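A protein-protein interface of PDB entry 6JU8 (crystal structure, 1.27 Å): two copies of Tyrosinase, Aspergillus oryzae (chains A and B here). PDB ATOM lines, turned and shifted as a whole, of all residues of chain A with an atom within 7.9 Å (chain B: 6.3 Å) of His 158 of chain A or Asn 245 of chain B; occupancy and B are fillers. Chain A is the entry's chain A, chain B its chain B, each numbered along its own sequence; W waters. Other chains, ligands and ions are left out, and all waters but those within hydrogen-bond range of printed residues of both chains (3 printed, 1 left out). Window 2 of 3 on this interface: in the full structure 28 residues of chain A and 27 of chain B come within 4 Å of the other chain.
Leu 31 of chain A touches Asn 247 of chain B.
His 158 of chain A touches Asn 245 of chain B (ND1 to ND2, 3.7 Å).
Glu 167 of chain A touches Arg 346 of chain B.
Printed residues of chain B within 4 Å of Leu 31 of chain A: Asn 247.
His 158 of chain A touches one residue of chain B.
Printed residues of chain B within 4 Å of Asp 166 of chain A: Arg 346 (2.7 Å).
Printed residues of chain B within 4 Å of Arg 169 of chain A: Asn 245 and Tyr 246.
Leu 243 of chain B touches none of the printed residues of chain A.
Of the printed residues of chain A, Asn 247 of chain B touches Leu 31.
Trp 251 of chain B touches none of the printed residues of chain A.
Of the printed residues of chain A, Arg 346 of chain B touches Asp 166 (2.7 Å) and Glu 167 (3.8 Å).
The nearest residue of chain A that does not touch Asn 245 of chain B is Arg 157 of chain A (4.4 Å).
The nearest printed residue of chain A that does not touch Tyr 246 of chain B is His 158 of chain A (6.2 Å).
OD2 of Asp 166 of chain A lies within salt-bridge range of NE of Arg 346 of chain B, 2.7 Å away.
OE1 of Glu 167 of chain A sits at hydrogen-bond distance from OH of Tyr 246 of chain B, at 2.6 Å.
NH2 of Arg 169 of chain A sits at hydrogen-bond distance from O of Asn 245 of chain B (3.1 Å).
OH of Tyr 246 of chain B sits at hydrogen-bond distance from NE of Arg 169 of chain A (3.3 Å).
The backbone NH (N) of Ala 156 of chain A lies within hydrogen-bond range of the backbone carbonyl oxygen (O) of Glu 167 of chain A (2.9 Å).
A ring nitrogen (NE2) of His 158 of chain A is in hydrogen-bond range of the side-chain carboxylate (OD1) of Asp 166 of chain A (3.1 Å).
The guanidinium group of Arg 169 of chain A lies within hydrogen-bond range of a ring nitrogen (NE2) of His 158 of chain A, 3.4 Å away.
The side-chain carboxylate (OE1) of Glu 167 of chain A is in salt-bridge range of the guanidinium group (NE) of Arg 169 of chain A.
No position is printed for both chains.
Of the 7 pairs that touch across the chains among the printed residues, none has its exchanged pair printed and touching as well.
Water W1 lies within hydrogen-bond range of N of Gly 159 of chain A, O of Asn 245 of chain B and O of Arg 157 of chain A.
Water W2 lies within hydrogen-bond range of the side-chain carboxylate (OE2) of Glu 167 of chain A and the side-chain hydroxyl (OH) of Tyr 246 of chain B.
Water W3 bridges the backbone NH (N) of Asn 247 of chain B (2.9 Å) and the guanidinium group (NH1) of Arg 169 of chain A (3.1 Å).
Hydrophobic or aromatic side chains of chain B within 4 Å of the printed part of chain A: Tyr 246.
Among the printed residues, 7 pairs touch across the chains.
Among the printed residues, Asp or Glu carboxylates within 4 Å of a Lys or Arg side-chain nitrogen of the other chain: Asp 166 of chain A with Arg 346 of chain B.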
ATOM      1  N   LEU A  31       8.677   1.025 -17.858  1.00  0.00           N
ATOM      2  CA  LEU A  31       8.984   0.621 -19.241  1.00  0.00           C
ATOM      3  C   LEU A  31      10.179   1.394 -19.762  1.00  0.00           C
ATOM      4  O   LEU A  31      10.992   0.820 -20.494  1.00  0.00           O
ATOM      5  CB  LEU A  31       7.747   0.838 -20.132  1.00  0.00           C
ATOM      6  CG  LEU A  31       6.530  -0.007 -19.715  1.00  0.00           C
ATOM      7  CD1 LEU A  31       5.300   0.346 -20.526  1.00  0.00           C
ATOM      8  CD2 LEU A  31       6.815  -1.501 -19.806  1.00  0.00           C
ATOM      9  N   PHE A 155      -5.935   4.132 -18.423  1.00  0.00           N
ATOM     10  CA  PHE A 155      -5.917   2.747 -18.880  1.00  0.00           C
ATOM     11  C   PHE A 155      -4.478   2.294 -19.064  1.00  0.00           C
ATOM     12  O   PHE A 155      -3.671   3.017 -19.669  1.00  0.00           O
ATOM     13  CB  PHE A 155      -6.665   2.660 -20.218  1.00  0.00           C
ATOM     14  CG  PHE A 155      -8.138   2.967 -20.093  1.00  0.00           C
ATOM     15  CD1 PHE A 155      -8.903   2.458 -19.049  1.00  0.00           C
ATOM     16  CD2 PHE A 155      -8.765   3.774 -21.035  1.00  0.00           C
ATOM     17  CE1 PHE A 155     -10.260   2.722 -19.007  1.00  0.00           C
ATOM     18  CE2 PHE A 155     -10.130   4.028 -21.004  1.00  0.00           C
ATOM     19  CZ  PHE A 155     -10.887   3.497 -19.977  1.00  0.00           C
ATOM     20  N   ALA A 156      -4.129   1.113 -18.550  1.00  0.00           N
ATOM     21  CA  ALA A 156      -2.792   0.563 -18.701  1.00  0.00           C
ATOM     22  C   ALA A 156      -2.470   0.300 -20.168  1.00  0.00           C
ATOM     23  O   ALA A 156      -3.338  -0.110 -20.938  1.00  0.00           O
ATOM     24  CB  ALA A 156      -2.685  -0.775 -17.968  1.00  0.00           C
ATOM     25  N   ARG A 157      -1.228   0.531 -20.579  1.00  0.00           N
ATOM     26  CA  ARG A 157      -0.916   0.359 -21.998  1.00  0.00           C
ATOM     27  C   ARG A 157      -0.653  -1.120 -22.262  1.00  0.00           C
ATOM     28  O   ARG A 157      -0.299  -1.875 -21.350  1.00  0.00           O
ATOM     29  CB  ARG A 157       0.276   1.237 -22.350  1.00  0.00           C
ATOM     30  CG  ARG A 157      -0.054   2.697 -22.615  1.00  0.00           C
ATOM     31  CD  ARG A 157      -0.633   3.396 -21.396  1.00  0.00           C
ATOM     32  NE  ARG A 157       0.386   3.688 -20.391  1.00  0.00           N
ATOM     33  CZ  ARG A 157       0.151   3.853 -19.088  1.00  0.00           C
ATOM     34  NH1 ARG A 157      -1.097   3.739 -18.632  1.00  0.00           N
ATOM     35  NH2 ARG A 157       1.125   4.119 -18.225  1.00  0.00           N
ATOM     36  N   HIS A 158      -0.846  -1.521 -23.503  1.00  0.00           N
ATOM     37  CA  HIS A 158      -0.579  -2.881 -23.968  1.00  0.00           C
ATOM     38  C   HIS A 158       0.740  -2.912 -24.729  1.00  0.00           C
ATOM     39  O   HIS A 158       0.814  -2.524 -25.900  1.00  0.00           O
ATOM     40  CB  HIS A 158      -1.731  -3.379 -24.846  1.00  0.00           C
ATOM     41  CG  HIS A 158      -3.033  -3.502 -24.113  1.00  0.00           C
ATOM     42  ND1 HIS A 158      -4.209  -3.869 -24.711  1.00  0.00           N
ATOM     43  CD2 HIS A 158      -3.342  -3.277 -22.813  1.00  0.00           C
ATOM     44  CE1 HIS A 158      -5.188  -3.887 -23.818  1.00  0.00           C
ATOM     45  NE2 HIS A 158      -4.684  -3.522 -22.649  1.00  0.00           N
ATOM     46  N   GLY A 159       1.800  -3.369 -24.072  1.00  0.00           N
ATOM     47  CA  GLY A 159       3.119  -3.375 -24.676  1.00  0.00           C
ATOM     48  C   GLY A 159       3.637  -1.966 -24.897  1.00  0.00           C
ATOM     49  O   GLY A 159       4.842  -1.769 -25.036  1.00  0.00           O
ATOM     50  N   GLY A 165      -4.800   0.927 -24.103  1.00  0.00           N
ATOM     51  CA  GLY A 165      -5.393  -0.075 -23.224  1.00  0.00           C
ATOM     52  C   GLY A 165      -6.864   0.172 -22.940  1.00  0.00           C
ATOM     53  O   GLY A 165      -7.445   1.167 -23.368  1.00  0.00           O
ATOM     54  N   ASP A 166      -7.491  -0.717 -22.191  1.00  0.00           N
ATOM     55  CA  ASP A 166      -8.924  -0.794 -22.009  1.00  0.00           C
ATOM     56  C   ASP A 166      -9.309  -0.932 -20.541  1.00  0.00           C
ATOM     57  O   ASP A 166     -10.493  -0.918 -20.193  1.00  0.00           O
ATOM     58  CB  ASP A 166      -9.441  -2.007 -22.800  1.00  0.00           C
ATOM     59  CG  ASP A 166      -8.818  -3.332 -22.405  1.00  0.00           C
ATOM     60  OD1 ASP A 166      -7.690  -3.365 -21.860  1.00  0.00           O
ATOM     61  OD2 ASP A 166      -9.471  -4.385 -22.653  1.00  0.00           O
ATOM     62  N   GLU A 167      -8.337  -1.159 -19.658  1.00  0.00           N
ATOM     63  CA  GLU A 167      -8.378  -1.652 -18.289  1.00  0.00           C
ATOM     64  C   GLU A 167      -7.562  -0.772 -17.341  1.00  0.00           C
ATOM     65  O   GLU A 167      -6.377  -0.518 -17.627  1.00  0.00           O
ATOM     66  CB  GLU A 167      -7.803  -3.086 -18.184  1.00  0.00           C
ATOM     67  CG  GLU A 167      -8.042  -3.782 -16.860  1.00  0.00           C
ATOM     68  CD  GLU A 167      -7.294  -5.066 -16.581  1.00  0.00           C
ATOM     69  OE1 GLU A 167      -6.336  -5.445 -17.290  1.00  0.00           O
ATOM     70  OE2 GLU A 167      -7.639  -5.778 -15.594  1.00  0.00           O
ATOM     71  N   ARG A 169      -5.319  -0.654 -13.997  1.00  0.00           N
ATOM     72  CA  ARG A 169      -4.544  -1.730 -13.393  1.00  0.00           C
ATOM     73  C   ARG A 169      -3.656  -1.195 -12.285  1.00  0.00           C
ATOM     74  O   ARG A 169      -3.139  -0.068 -12.379  1.00  0.00           O
ATOM     75  CB  ARG A 169      -3.601  -2.394 -14.406  1.00  0.00           C
ATOM     76  CG  ARG A 169      -4.316  -3.088 -15.574  1.00  0.00           C
ATOM     77  CD  ARG A 169      -3.249  -3.780 -16.424  1.00  0.00           C
ATOM     78  NE  ARG A 169      -3.791  -4.223 -17.712  1.00  0.00           N
ATOM     79  CZ  ARG A 169      -2.998  -4.620 -18.703  1.00  0.00           C
ATOM     80  NH1 ARG A 169      -1.674  -4.591 -18.532  1.00  0.00           N
ATOM     81  NH2 ARG A 169      -3.543  -5.024 -19.846  1.00  0.00           N
ATOM     82  N   ILE A 172       2.523  -2.196 -12.985  1.00  0.00           N
ATOM     83  CA  ILE A 172       3.303  -3.387 -13.345  1.00  0.00           C
ATOM     84  C   ILE A 172       4.202  -3.807 -12.191  1.00  0.00           C
ATOM     85  O   ILE A 172       4.214  -4.963 -11.741  1.00  0.00           O
ATOM     86  CB  ILE A 172       4.148  -3.132 -14.605  1.00  0.00           C
ATOM     87  CG1 ILE A 172       3.303  -2.794 -15.848  1.00  0.00           C
ATOM     88  CG2 ILE A 172       5.039  -4.321 -14.889  1.00  0.00           C
ATOM     89  CD1 ILE A 172       4.080  -2.106 -16.957  1.00  0.00           C
ATOM     90  N   LEU B 243      -1.969 -13.327 -18.034  1.00  0.00           N
ATOM     91  CA  LEU B 243      -3.046 -12.639 -18.759  1.00  0.00           C
ATOM     92  C   LEU B 243      -2.452 -12.017 -20.013  1.00  0.00           C
ATOM     93  O   LEU B 243      -1.339 -11.466 -19.975  1.00  0.00           O
ATOM     94  CB  LEU B 243      -3.681 -11.524 -17.936  1.00  0.00           C
ATOM     95  CG  LEU B 243      -4.638 -11.878 -16.783  1.00  0.00           C
ATOM     96  CD1 LEU B 243      -3.972 -12.698 -15.691  1.00  0.00           C
ATOM     97  CD2 LEU B 243      -5.180 -10.580 -16.174  1.00  0.00           C
ATOM     98  N   GLU B 244      -3.216 -12.074 -21.098  1.00  0.00           N
ATOM     99  CA  GLU B 244      -2.769 -11.449 -22.343  1.00  0.00           C
ATOM    100  C   GLU B 244      -2.590  -9.950 -22.178  1.00  0.00           C
ATOM    101  O   GLU B 244      -3.380  -9.306 -21.474  1.00  0.00           O
ATOM    102  CB  GLU B 244      -3.798 -11.707 -23.458  1.00  0.00           C
ATOM    103  CG  GLU B 244      -3.174 -11.427 -24.820  1.00  0.00           C
ATOM    104  CD  GLU B 244      -4.096 -11.672 -25.980  1.00  0.00           C
ATOM    105  OE1 GLU B 244      -3.589 -11.872 -27.121  1.00  0.00           O
ATOM    106  OE2 GLU B 244      -5.330 -11.680 -25.783  1.00  0.00           O
ATOM    107  N   ASN B 245      -1.617  -9.375 -22.870  1.00  0.00           N
ATOM    108  CA  ASN B 245      -1.373  -7.936 -22.863  1.00  0.00           C
ATOM    109  C   ASN B 245      -0.888  -7.436 -21.510  1.00  0.00           C
ATOM    110  O   ASN B 245      -1.054  -6.249 -21.202  1.00  0.00           O
ATOM    111  CB  ASN B 245      -2.594  -7.137 -23.336  1.00  0.00           C
ATOM    112  CG  ASN B 245      -2.890  -7.433 -24.801  1.00  0.00           C
ATOM    113  OD1 ASN B 245      -1.965  -7.575 -25.594  1.00  0.00           O
ATOM    114  ND2 ASN B 245      -4.155  -7.577 -25.179  1.00  0.00           N
ATOM    115  N   TYR B 246      -0.256  -8.295 -20.731  1.00  0.00           N
ATOM    116  CA  TYR B 246       0.484  -7.914 -19.532  1.00  0.00           C
ATOM    117  C   TYR B 246       1.975  -8.059 -19.826  1.00  0.00           C
ATOM    118  O   TYR B 246       2.381  -8.962 -20.557  1.00  0.00           O
ATOM    119  CB  TYR B 246       0.076  -8.773 -18.330  1.00  0.00           C
ATOM    120  CG  TYR B 246      -1.199  -8.257 -17.682  1.00  0.00           C
ATOM    121  CD1 TYR B 246      -1.192  -7.739 -16.393  1.00  0.00           C
ATOM    122  CD2 TYR B 246      -2.402  -8.256 -18.365  1.00  0.00           C
ATOM    123  CE1 TYR B 246      -2.353  -7.252 -15.808  1.00  0.00           C
ATOM    124  CE2 TYR B 246      -3.575  -7.776 -17.808  1.00  0.00           C
ATOM    125  CZ  TYR B 246      -3.535  -7.273 -16.519  1.00  0.00           C
ATOM    126  OH  TYR B 246      -4.667  -6.790 -15.887  1.00  0.00           O
ATOM    127  N   ASN B 247       2.747  -7.154 -19.245  1.00  0.00           N
ATOM    128  CA  ASN B 247       4.209  -7.173 -19.383  1.00  0.00           C
ATOM    129  C   ASN B 247       4.764  -8.535 -19.002  1.00  0.00           C
ATOM    130  O   ASN B 247       4.334  -9.095 -17.988  1.00  0.00           O
ATOM    131  CB  ASN B 247       4.792  -6.072 -18.498  1.00  0.00           C
ATOM    132  CG  ASN B 247       6.289  -5.899 -18.664  1.00  0.00           C
ATOM    133  OD1 ASN B 247       7.104  -6.743 -18.261  1.00  0.00           O
ATOM    134  ND2 ASN B 247       6.642  -4.762 -19.233  1.00  0.00           N
ATOM    135  N   TRP B 251       4.666 -12.195 -15.886  1.00  0.00           N
ATOM    136  CA  TRP B 251       4.570 -13.620 -16.165  1.00  0.00           C
ATOM    137  C   TRP B 251       5.684 -14.423 -15.492  1.00  0.00           C
ATOM    138  O   TRP B 251       5.527 -15.631 -15.286  1.00  0.00           O
ATOM    139  CB  TRP B 251       4.628 -13.834 -17.682  1.00  0.00           C
ATOM    140  CG  TRP B 251       3.461 -13.283 -18.452  1.00  0.00           C
ATOM    141  CD1 TRP B 251       2.264 -12.818 -18.001  1.00  0.00           C
ATOM    142  CD2 TRP B 251       3.435 -13.150 -19.887  1.00  0.00           C
ATOM    143  NE1 TRP B 251       1.488 -12.414 -19.062  1.00  0.00           N
ATOM    144  CE2 TRP B 251       2.187 -12.604 -20.235  1.00  0.00           C
ATOM    145  CE3 TRP B 251       4.358 -13.441 -20.895  1.00  0.00           C
ATOM    146  CZ2 TRP B 251       1.831 -12.348 -21.555  1.00  0.00           C
ATOM    147  CZ3 TRP B 251       4.006 -13.191 -22.224  1.00  0.00           C
ATOM    148  CH2 TRP B 251       2.752 -12.645 -22.535  1.00  0.00           C
ATOM    149  N   PHE B 344      -6.576 -17.081 -20.690  1.00  0.00           N
ATOM    150  CA  PHE B 344      -5.447 -16.178 -20.885  1.00  0.00           C
ATOM    151  C   PHE B 344      -5.949 -14.881 -21.496  1.00  0.00           C
ATOM    152  O   PHE B 344      -5.607 -13.771 -21.079  1.00  0.00           O
ATOM    153  CB  PHE B 344      -4.424 -16.894 -21.760  1.00  0.00           C
ATOM    154  CG  PHE B 344      -3.216 -16.079 -22.148  1.00  0.00           C
ATOM    155  CD1 PHE B 344      -2.303 -15.612 -21.224  1.00  0.00           C
ATOM    156  CD2 PHE B 344      -2.998 -15.775 -23.496  1.00  0.00           C
ATOM    157  CE1 PHE B 344      -1.186 -14.864 -21.592  1.00  0.00           C
ATOM    158  CE2 PHE B 344      -1.878 -15.056 -23.878  1.00  0.00           C
ATOM    159  CZ  PHE B 344      -0.967 -14.603 -22.940  1.00  0.00           C
ATOM    160  N   ARG B 346      -8.511 -11.898 -22.511  1.00  0.00           N
ATOM    161  CA  ARG B 346      -9.537 -11.201 -21.742  1.00  0.00           C
ATOM    162  C   ARG B 346     -10.910 -11.678 -22.182  1.00  0.00           C
ATOM    163  O   ARG B 346     -11.225 -11.630 -23.368  1.00  0.00           O
ATOM    164  CB  ARG B 346      -9.398  -9.698 -21.947  1.00  0.00           C
ATOM    165  CG  ARG B 346     -10.132  -8.791 -20.961  1.00  0.00           C
ATOM    166  CD  ARG B 346      -9.583  -7.375 -21.072  1.00  0.00           C
ATOM    167  NE  ARG B 346     -10.615  -6.355 -21.164  1.00  0.00           N
ATOM    168  CZ  ARG B 346     -11.027  -5.648 -20.117  1.00  0.00           C
ATOM    169  NH1 ARG B 346     -10.482  -5.861 -18.923  1.00  0.00           N
ATOM    170  NH2 ARG B 346     -11.967  -4.732 -20.255  1.00  0.00           N
HETATM  171  O   HOH W   1       1.476  -4.797 -21.868  1.00  0.00           O
HETATM  172  O   HOH W   2      -6.668  -7.934 -14.176  1.00  0.00           O
HETATM  173  O   HOH W   3       1.402  -4.906 -18.062  1.00  0.00           O
